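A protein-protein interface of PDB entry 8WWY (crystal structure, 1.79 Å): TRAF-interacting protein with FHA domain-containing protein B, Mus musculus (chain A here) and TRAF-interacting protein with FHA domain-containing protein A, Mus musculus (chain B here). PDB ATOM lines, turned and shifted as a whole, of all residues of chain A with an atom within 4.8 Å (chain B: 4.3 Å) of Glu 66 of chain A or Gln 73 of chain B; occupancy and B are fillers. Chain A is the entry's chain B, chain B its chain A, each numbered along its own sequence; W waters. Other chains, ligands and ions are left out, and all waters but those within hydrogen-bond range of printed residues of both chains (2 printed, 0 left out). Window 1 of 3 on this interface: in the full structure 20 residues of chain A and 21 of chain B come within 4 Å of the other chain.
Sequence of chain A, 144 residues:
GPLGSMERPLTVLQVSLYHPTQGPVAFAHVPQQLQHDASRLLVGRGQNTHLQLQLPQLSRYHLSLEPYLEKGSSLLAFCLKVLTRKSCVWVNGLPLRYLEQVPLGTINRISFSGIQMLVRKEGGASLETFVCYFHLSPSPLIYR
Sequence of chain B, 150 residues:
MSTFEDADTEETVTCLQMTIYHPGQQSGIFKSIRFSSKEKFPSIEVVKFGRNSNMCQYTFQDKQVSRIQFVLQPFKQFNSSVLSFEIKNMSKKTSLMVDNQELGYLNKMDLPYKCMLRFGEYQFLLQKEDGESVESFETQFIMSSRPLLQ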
ATOM      1  N   ARG A  40     -33.921  -6.923  17.032  1.00  0.00           N
ATOM      2  CA  ARG A  40     -33.140  -7.956  16.367  1.00  0.00           C
ATOM      3  C   ARG A  40     -33.878  -9.290  16.406  1.00  0.00           C
ATOM      4  O   ARG A  40     -34.647  -9.586  17.326  1.00  0.00           O
ATOM      5  CB  ARG A  40     -31.754  -8.104  17.006  1.00  0.00           C
ATOM      6  CG  ARG A  40     -31.776  -8.659  18.426  1.00  0.00           C
ATOM      7  CD  ARG A  40     -30.357  -8.763  18.975  1.00  0.00           C
ATOM      8  NE  ARG A  40     -30.355  -9.265  20.343  1.00  0.00           N
ATOM      9  CZ  ARG A  40     -29.258  -9.645  20.990  1.00  0.00           C
ATOM     10  NH1 ARG A  40     -28.075  -9.592  20.384  1.00  0.00           N
ATOM     11  NH2 ARG A  40     -29.348 -10.094  22.240  1.00  0.00           N
ATOM     12  N   SER A  64     -27.738 -13.050  14.555  1.00  0.00           N
ATOM     13  CA  SER A  64     -28.910 -12.183  14.613  1.00  0.00           C
ATOM     14  C   SER A  64     -29.084 -11.438  13.299  1.00  0.00           C
ATOM     15  O   SER A  64     -28.121 -11.210  12.560  1.00  0.00           O
ATOM     16  CB  SER A  64     -28.819 -11.168  15.771  1.00  0.00           C
ATOM     17  OG  SER A  64     -27.678 -10.345  15.630  1.00  0.00           O
ATOM     18  N   LEU A  65     -30.335 -11.084  13.009  1.00  0.00           N
ATOM     19  CA  LEU A  65     -30.706 -10.218  11.893  1.00  0.00           C
ATOM     20  C   LEU A  65     -31.302  -8.951  12.487  1.00  0.00           C
ATOM     21  O   LEU A  65     -32.312  -9.017  13.197  1.00  0.00           O
ATOM     22  CB  LEU A  65     -31.722 -10.899  10.965  1.00  0.00           C
ATOM     23  CG  LEU A  65     -31.268 -12.182  10.264  1.00  0.00           C
ATOM     24  CD1 LEU A  65     -32.455 -12.773   9.496  1.00  0.00           C
ATOM     25  CD2 LEU A  65     -30.123 -11.926   9.323  1.00  0.00           C
ATOM     26  N   GLU A  66     -30.661  -7.808  12.222  1.00  0.00           N
ATOM     27  CA  GLU A  66     -31.061  -6.533  12.816  1.00  0.00           C
ATOM     28  C   GLU A  66     -31.629  -5.613  11.752  1.00  0.00           C
ATOM     29  O   GLU A  66     -30.884  -5.237  10.834  1.00  0.00           O
ATOM     30  CB  GLU A  66     -29.863  -5.848  13.490  1.00  0.00           C
ATOM     31  CG  GLU A  66     -30.195  -4.437  13.947  1.00  0.00           C
ATOM     32  CD  GLU A  66     -29.077  -3.430  13.662  1.00  0.00           C
ATOM     33  OE1 GLU A  66     -28.003  -3.853  13.196  1.00  0.00           O
ATOM     34  OE2 GLU A  66     -29.284  -2.215  13.901  1.00  0.00           O
ATOM     35  N   PRO A  67     -32.895  -5.188  11.847  1.00  0.00           N
ATOM     36  CA  PRO A  67     -33.416  -4.207  10.893  1.00  0.00           C
ATOM     37  C   PRO A  67     -33.002  -2.801  11.303  1.00  0.00           C
ATOM     38  O   PRO A  67     -32.950  -2.473  12.490  1.00  0.00           O
ATOM     39  CB  PRO A  67     -34.933  -4.393  11.003  1.00  0.00           C
ATOM     40  CG  PRO A  67     -35.132  -4.728  12.471  1.00  0.00           C
ATOM     41  CD  PRO A  67     -33.908  -5.568  12.852  1.00  0.00           C
ATOM     42  N   TYR A  68     -32.688  -1.977  10.309  1.00  0.00           N
ATOM     43  CA  TYR A  68     -32.299  -0.596  10.571  1.00  0.00           C
ATOM     44  C   TYR A  68     -32.529   0.212   9.305  1.00  0.00           C
ATOM     45  O   TYR A  68     -32.894  -0.328   8.258  1.00  0.00           O
ATOM     46  CB  TYR A  68     -30.839  -0.500  11.037  1.00  0.00           C
ATOM     47  CG  TYR A  68     -29.801  -0.825   9.968  1.00  0.00           C
ATOM     48  CD1 TYR A  68     -29.505  -2.138   9.635  1.00  0.00           C
ATOM     49  CD2 TYR A  68     -29.095   0.189   9.312  1.00  0.00           C
ATOM     50  CE1 TYR A  68     -28.557  -2.442   8.660  1.00  0.00           C
ATOM     51  CE2 TYR A  68     -28.140  -0.109   8.343  1.00  0.00           C
ATOM     52  CZ  TYR A  68     -27.880  -1.428   8.027  1.00  0.00           C
ATOM     53  OH  TYR A  68     -26.937  -1.763   7.083  1.00  0.00           O
ATOM     54  N   ALA A  77     -32.958  -1.906   5.942  1.00  0.00           N
ATOM     55  CA  ALA A  77     -31.775  -2.726   5.722  1.00  0.00           C
ATOM     56  C   ALA A  77     -31.681  -3.753   6.838  1.00  0.00           C
ATOM     57  O   ALA A  77     -32.361  -3.653   7.864  1.00  0.00           O
ATOM     58  CB  ALA A  77     -30.503  -1.869   5.668  1.00  0.00           C
ATOM     59  N   PHE A  78     -30.838  -4.764   6.625  1.00  0.00           N
ATOM     60  CA  PHE A  78     -30.700  -5.850   7.576  1.00  0.00           C
ATOM     61  C   PHE A  78     -29.234  -6.172   7.767  1.00  0.00           C
ATOM     62  O   PHE A  78     -28.503  -6.368   6.791  1.00  0.00           O
ATOM     63  CB  PHE A  78     -31.458  -7.098   7.113  1.00  0.00           C
ATOM     64  CG  PHE A  78     -32.926  -6.872   7.036  1.00  0.00           C
ATOM     65  CD1 PHE A  78     -33.473  -6.286   5.914  1.00  0.00           C
ATOM     66  CD2 PHE A  78     -33.746  -7.176   8.108  1.00  0.00           C
ATOM     67  CE1 PHE A  78     -34.844  -6.027   5.842  1.00  0.00           C
ATOM     68  CE2 PHE A  78     -35.111  -6.933   8.041  1.00  0.00           C
ATOM     69  CZ  PHE A  78     -35.656  -6.357   6.909  1.00  0.00           C
ATOM     70  N   CYS A  79     -28.826  -6.214   9.032  1.00  0.00           N
ATOM     71  CA  CYS A  79     -27.451  -6.469   9.438  1.00  0.00           C
ATOM     72  C   CYS A  79     -27.394  -7.851  10.079  1.00  0.00           C
ATOM     73  O   CYS A  79     -28.075  -8.096  11.081  1.00  0.00           O
ATOM     74  CB  CYS A  79     -26.991  -5.390  10.423  1.00  0.00           C
ATOM     75  SG  CYS A  79     -25.358  -5.697  11.112  1.00  0.00           S
ATOM     76  N   LYS A  81     -25.264 -10.321  12.219  1.00  0.00           N
ATOM     77  CA  LYS A  81     -24.131 -10.356  13.134  1.00  0.00           C
ATOM     78  C   LYS A  81     -23.977 -11.748  13.727  1.00  0.00           C
ATOM     79  O   LYS A  81     -24.968 -12.396  14.086  1.00  0.00           O
ATOM     80  CB  LYS A  81     -24.296  -9.328  14.268  1.00  0.00           C
ATOM     81  CG  LYS A  81     -23.097  -9.317  15.227  1.00  0.00           C
ATOM     82  CD  LYS A  81     -23.064  -8.024  16.063  1.00  0.00           C
ATOM     83  CE  LYS A  81     -24.289  -7.882  16.948  1.00  0.00           C
ATOM     84  NZ  LYS A  81     -24.410  -6.480  17.464  1.00  0.00           N
ATOM     85  N   VAL B  71     -30.592   2.090  21.734  1.00  0.00           N
ATOM     86  CA  VAL B  71     -29.987   0.817  22.092  1.00  0.00           C
ATOM     87  C   VAL B  71     -28.506   0.881  21.757  1.00  0.00           C
ATOM     88  O   VAL B  71     -28.091   1.566  20.817  1.00  0.00           O
ATOM     89  CB  VAL B  71     -30.667  -0.368  21.364  1.00  0.00           C
ATOM     90  CG1 VAL B  71     -32.140  -0.460  21.776  1.00  0.00           C
ATOM     91  CG2 VAL B  71     -30.544  -0.209  19.841  1.00  0.00           C
ATOM     92  N   LEU B  72     -27.707   0.158  22.536  1.00  0.00           N
ATOM     93  CA  LEU B  72     -26.289  -0.028  22.266  1.00  0.00           C
ATOM     94  C   LEU B  72     -26.074  -1.435  21.718  1.00  0.00           C
ATOM     95  O   LEU B  72     -26.548  -2.415  22.309  1.00  0.00           O
ATOM     96  CB  LEU B  72     -25.457   0.205  23.532  1.00  0.00           C
ATOM     97  CG  LEU B  72     -25.606   1.597  24.158  1.00  0.00           C
ATOM     98  CD1 LEU B  72     -24.838   1.702  25.474  1.00  0.00           C
ATOM     99  CD2 LEU B  72     -25.143   2.672  23.174  1.00  0.00           C
ATOM    100  N   GLN B  73     -25.386  -1.526  20.581  1.00  0.00           N
ATOM    101  CA  GLN B  73     -25.192  -2.785  19.856  1.00  0.00           C
ATOM    102  C   GLN B  73     -23.703  -3.106  19.762  1.00  0.00           C
ATOM    103  O   GLN B  73     -22.991  -2.538  18.915  1.00  0.00           O
ATOM    104  CB  GLN B  73     -25.830  -2.703  18.465  1.00  0.00           C
ATOM    105  CG  GLN B  73     -27.355  -2.488  18.570  1.00  0.00           C
ATOM    106  CD  GLN B  73     -28.101  -2.318  17.248  1.00  0.00           C
ATOM    107  OE1 GLN B  73     -29.329  -2.455  17.213  1.00  0.00           O
ATOM    108  NE2 GLN B  73     -27.381  -1.998  16.170  1.00  0.00           N
ATOM    109  N   PRO B  74     -23.190  -3.991  20.612  1.00  0.00           N
ATOM    110  CA  PRO B  74     -21.759  -4.320  20.569  1.00  0.00           C
ATOM    111  C   PRO B  74     -21.412  -5.127  19.325  1.00  0.00           C
ATOM    112  O   PRO B  74     -22.164  -6.026  18.925  1.00  0.00           O
ATOM    113  CB  PRO B  74     -21.552  -5.159  21.838  1.00  0.00           C
ATOM    114  CG  PRO B  74     -22.810  -4.994  22.660  1.00  0.00           C
ATOM    115  CD  PRO B  74     -23.903  -4.725  21.673  1.00  0.00           C
ATOM    116  N   PHE B  75     -20.261  -4.816  18.726  1.00  0.00           N
ATOM    117  CA  PHE B  75     -19.821  -5.535  17.530  1.00  0.00           C
ATOM    118  C   PHE B  75     -18.308  -5.420  17.401  1.00  0.00           C
ATOM    119  O   PHE B  75     -17.658  -4.666  18.125  1.00  0.00           O
ATOM    120  CB  PHE B  75     -20.519  -5.002  16.271  1.00  0.00           C
ATOM    121  CG  PHE B  75     -19.958  -3.700  15.778  1.00  0.00           C
ATOM    122  CD1 PHE B  75     -20.264  -2.509  16.421  1.00  0.00           C
ATOM    123  CD2 PHE B  75     -19.118  -3.670  14.674  1.00  0.00           C
ATOM    124  CE1 PHE B  75     -19.728  -1.303  15.968  1.00  0.00           C
ATOM    125  CE2 PHE B  75     -18.589  -2.483  14.222  1.00  0.00           C
ATOM    126  CZ  PHE B  75     -18.901  -1.294  14.864  1.00  0.00           C
ATOM    127  N   SER B  84     -16.356  -2.709  19.688  1.00  0.00           N
ATOM    128  CA  SER B  84     -16.987  -1.456  19.294  1.00  0.00           C
ATOM    129  C   SER B  84     -18.465  -1.498  19.663  1.00  0.00           C
ATOM    130  O   SER B  84     -19.016  -2.548  20.005  1.00  0.00           O
ATOM    131  CB  SER B  84     -16.824  -1.196  17.794  1.00  0.00           C
ATOM    132  OG  SER B  84     -15.465  -1.025  17.449  1.00  0.00           O
ATOM    133  N   PHE B  85     -19.117  -0.339  19.580  1.00  0.00           N
ATOM    134  CA  PHE B  85     -20.539  -0.247  19.884  1.00  0.00           C
ATOM    135  C   PHE B  85     -21.216   0.666  18.879  1.00  0.00           C
ATOM    136  O   PHE B  85     -20.780   1.802  18.674  1.00  0.00           O
ATOM    137  CB  PHE B  85     -20.788   0.292  21.303  1.00  0.00           C
ATOM    138  CG  PHE B  85     -20.200  -0.571  22.390  1.00  0.00           C
ATOM    139  CD1 PHE B  85     -18.861  -0.448  22.744  1.00  0.00           C
ATOM    140  CD2 PHE B  85     -20.983  -1.510  23.050  1.00  0.00           C
ATOM    141  CE1 PHE B  85     -18.307  -1.242  23.734  1.00  0.00           C
ATOM    142  CE2 PHE B  85     -20.434  -2.314  24.043  1.00  0.00           C
ATOM    143  CZ  PHE B  85     -19.094  -2.172  24.391  1.00  0.00           C
ATOM    144  N   GLU B  86     -22.277   0.169  18.257  1.00  0.00           N
ATOM    145  CA  GLU B  86     -23.192   1.052  17.560  1.00  0.00           C
ATOM    146  C   GLU B  86     -24.197   1.611  18.553  1.00  0.00           C
ATOM    147  O   GLU B  86     -24.579   0.945  19.520  1.00  0.00           O
ATOM    148  CB  GLU B  86     -23.952   0.306  16.452  1.00  0.00           C
ATOM    149  CG  GLU B  86     -23.054  -0.335  15.410  1.00  0.00           C
ATOM    150  CD  GLU B  86     -23.826  -1.274  14.512  1.00  0.00           C
ATOM    151  OE1 GLU B  86     -24.769  -1.914  15.016  1.00  0.00           O
ATOM    152  OE2 GLU B  86     -23.491  -1.351  13.319  1.00  0.00           O
ATOM    153  N   LYS B  88     -28.137   3.168  18.188  1.00  0.00           N
ATOM    154  CA  LYS B  88     -29.231   3.262  17.236  1.00  0.00           C
ATOM    155  C   LYS B  88     -30.420   3.921  17.911  1.00  0.00           C
ATOM    156  O   LYS B  88     -30.801   3.539  19.023  1.00  0.00           O
ATOM    157  CB  LYS B  88     -29.630   1.883  16.682  1.00  0.00           C
ATOM    158  CG  LYS B  88     -30.759   1.965  15.648  1.00  0.00           C
ATOM    159  CD  LYS B  88     -30.893   0.668  14.839  1.00  0.00           C
ATOM    160  CE  LYS B  88     -31.632  -0.405  15.612  1.00  0.00           C
ATOM    161  NZ  LYS B  88     -31.708  -1.688  14.855  1.00  0.00           N
ATOM    162  N   LYS B 108     -28.400   4.310  12.802  1.00  0.00           N
ATOM    163  CA  LYS B 108     -27.348   3.907  13.730  1.00  0.00           C
ATOM    164  C   LYS B 108     -25.998   4.408  13.240  1.00  0.00           C
ATOM    165  O   LYS B 108     -25.837   4.783  12.080  1.00  0.00           O
ATOM    166  CB  LYS B 108     -27.298   2.372  13.916  1.00  0.00           C
ATOM    167  CG  LYS B 108     -26.964   1.581  12.652  1.00  0.00           C
ATOM    168  CD  LYS B 108     -26.732   0.099  12.993  1.00  0.00           C
ATOM    169  CE  LYS B 108     -26.397  -0.728  11.758  1.00  0.00           C
ATOM    170  NZ  LYS B 108     -25.973  -2.127  12.135  1.00  0.00           N
HETATM  171  O   HOH W   1     -24.550  -4.604  15.359  1.00  0.00           O
HETATM  172  O   HOH W   2     -24.975  -2.747   9.256  1.00  0.00           O
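Printed residues of chain B that touch a printed residue of chain A: Gln 73, Pro 74, Phe 75, Lys 88 and Lys 108.
Of the 10 printed residues of chain A, 5 touch a printed residue of chain B.
Printed residues of chain A that touch a printed residue of chain B: Glu 66, Pro 67, Tyr 68, Cys 79 and Lys 81.
Hydrophobic or aromatic side chains of chain A within 4 Å of the printed part of chain B: Tyr 68.
Among the printed residues, Asp or Glu carboxylates within 4 Å of a Lys or Arg side-chain nitrogen of the other chain: Glu 66 of chain A with Lys 88 of chain B (2.7 Å) and Glu 66 of chain A with Lys 108 of chain B (2.9 Å).
OE1 of Gln 73 of chain B sits at hydrogen-bond distance from NZ of Lys 88 of chain B (3.4 Å).
The backbone NH (N) of Ser 64 of chain A is in hydrogen-bond range of the backbone carbonyl oxygen (O) of Lys 81 of chain A (2.9 Å).
OE2 of Glu 86 of chain B is in salt-bridge range of NZ of Lys 108 of chain B, at 2.9 Å.
The backbone carbonyl oxygen of Phe 75 of chain B lies within hydrogen-bond range of the backbone NH of Ser 84 of chain B (2.8 Å).
The backbone carbonyl oxygen of Tyr 68 of chain A sits at hydrogen-bond distance from the backbone NH of Ala 77 of chain A, at 2.8 Å.
The backbone carbonyl oxygen (O) of Glu 86 of chain B sits at hydrogen-bond distance from the backbone NH (N) of Gln 73 of chain B, at 2.8 Å.
Among the printed residues, pairs that only touch across the chains: Tyr 68 of chain A with Lys 108 of chain B (3.8 Å), Lys 81 of chain A with Phe 75 of chain B (3.96 Å) and Tyr 68 of chain A with Lys 88 of chain B (3.98 Å).
Water W1 bridges OE1 of Glu 86 of chain B (2.7 Å) and NZ of Lys 81 of chain A (2.8 Å).
Water W2 lies within hydrogen-bond range of the side-chain hydroxyl of Tyr 68 of chain A (3.1 Å), the side-chain amino group of Lys 108 of chain B (3.1 Å) and the side-chain sulfur of Cys 79 of chain A (3.5 Å).
The side-chain amino group (NZ) of Lys 88 of chain B is in hydrogen-bond range of the backbone carbonyl oxygen (O) of Pro 67 of chain A (2.8 Å).
The side-chain amino group (NZ) of Lys 81 of chain A is in hydrogen-bond range of the backbone carbonyl oxygen (O) of Pro 74 of chain B, 2.7 Å away.
The side-chain sulfur (SG) of Cys 79 of chain A is in hydrogen-bond range of the side-chain amino group (NZ) of Lys 108 of chain B, 3.8 Å away.
OE1 of Glu 66 of chain A lies within salt-bridge range of NZ of Lys 108 of chain B (2.9 Å).
NZ of Lys 88 of chain B lies within salt-bridge range of OE2 of Glu 66 of chain A, at 2.7 Å.
The side-chain amide nitrogen of Gln 73 of chain B lies within hydrogen-bond range of the side-chain carboxylate of Glu 66 of chain A (3.0 Å).
Glu 66 of chain A touches just these residues of chain B: Gln 73, Lys 88 and Lys 108.
Of the printed residues of chain B, Tyr 68 of chain A touches Lys 88 and Lys 108.
Of chain A, only Glu 66 comes within 4 Å of Gln 73 of chain B.
Of the printed residues of chain A, Lys 88 of chain B touches Glu 66 (2.7 Å), Pro 67 (2.8 Å) and Tyr 68 (3.98 Å).
Printed residues of chain A within 4 Å of Lys 108 of chain B: Glu 66, Tyr 68 and Cys 79.
The nearest residue of chain B that does not touch Glu 66 of chain A is Glu 86 of chain B (4.2 Å).
The nearest residue of chain A that does not touch Gln 73 of chain B is Lys 81 of chain A (4.1 Å).
The nearest printed residue of chain A that does not touch Lys 108 of chain B is Pro 67 of chain A (6.7 Å).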
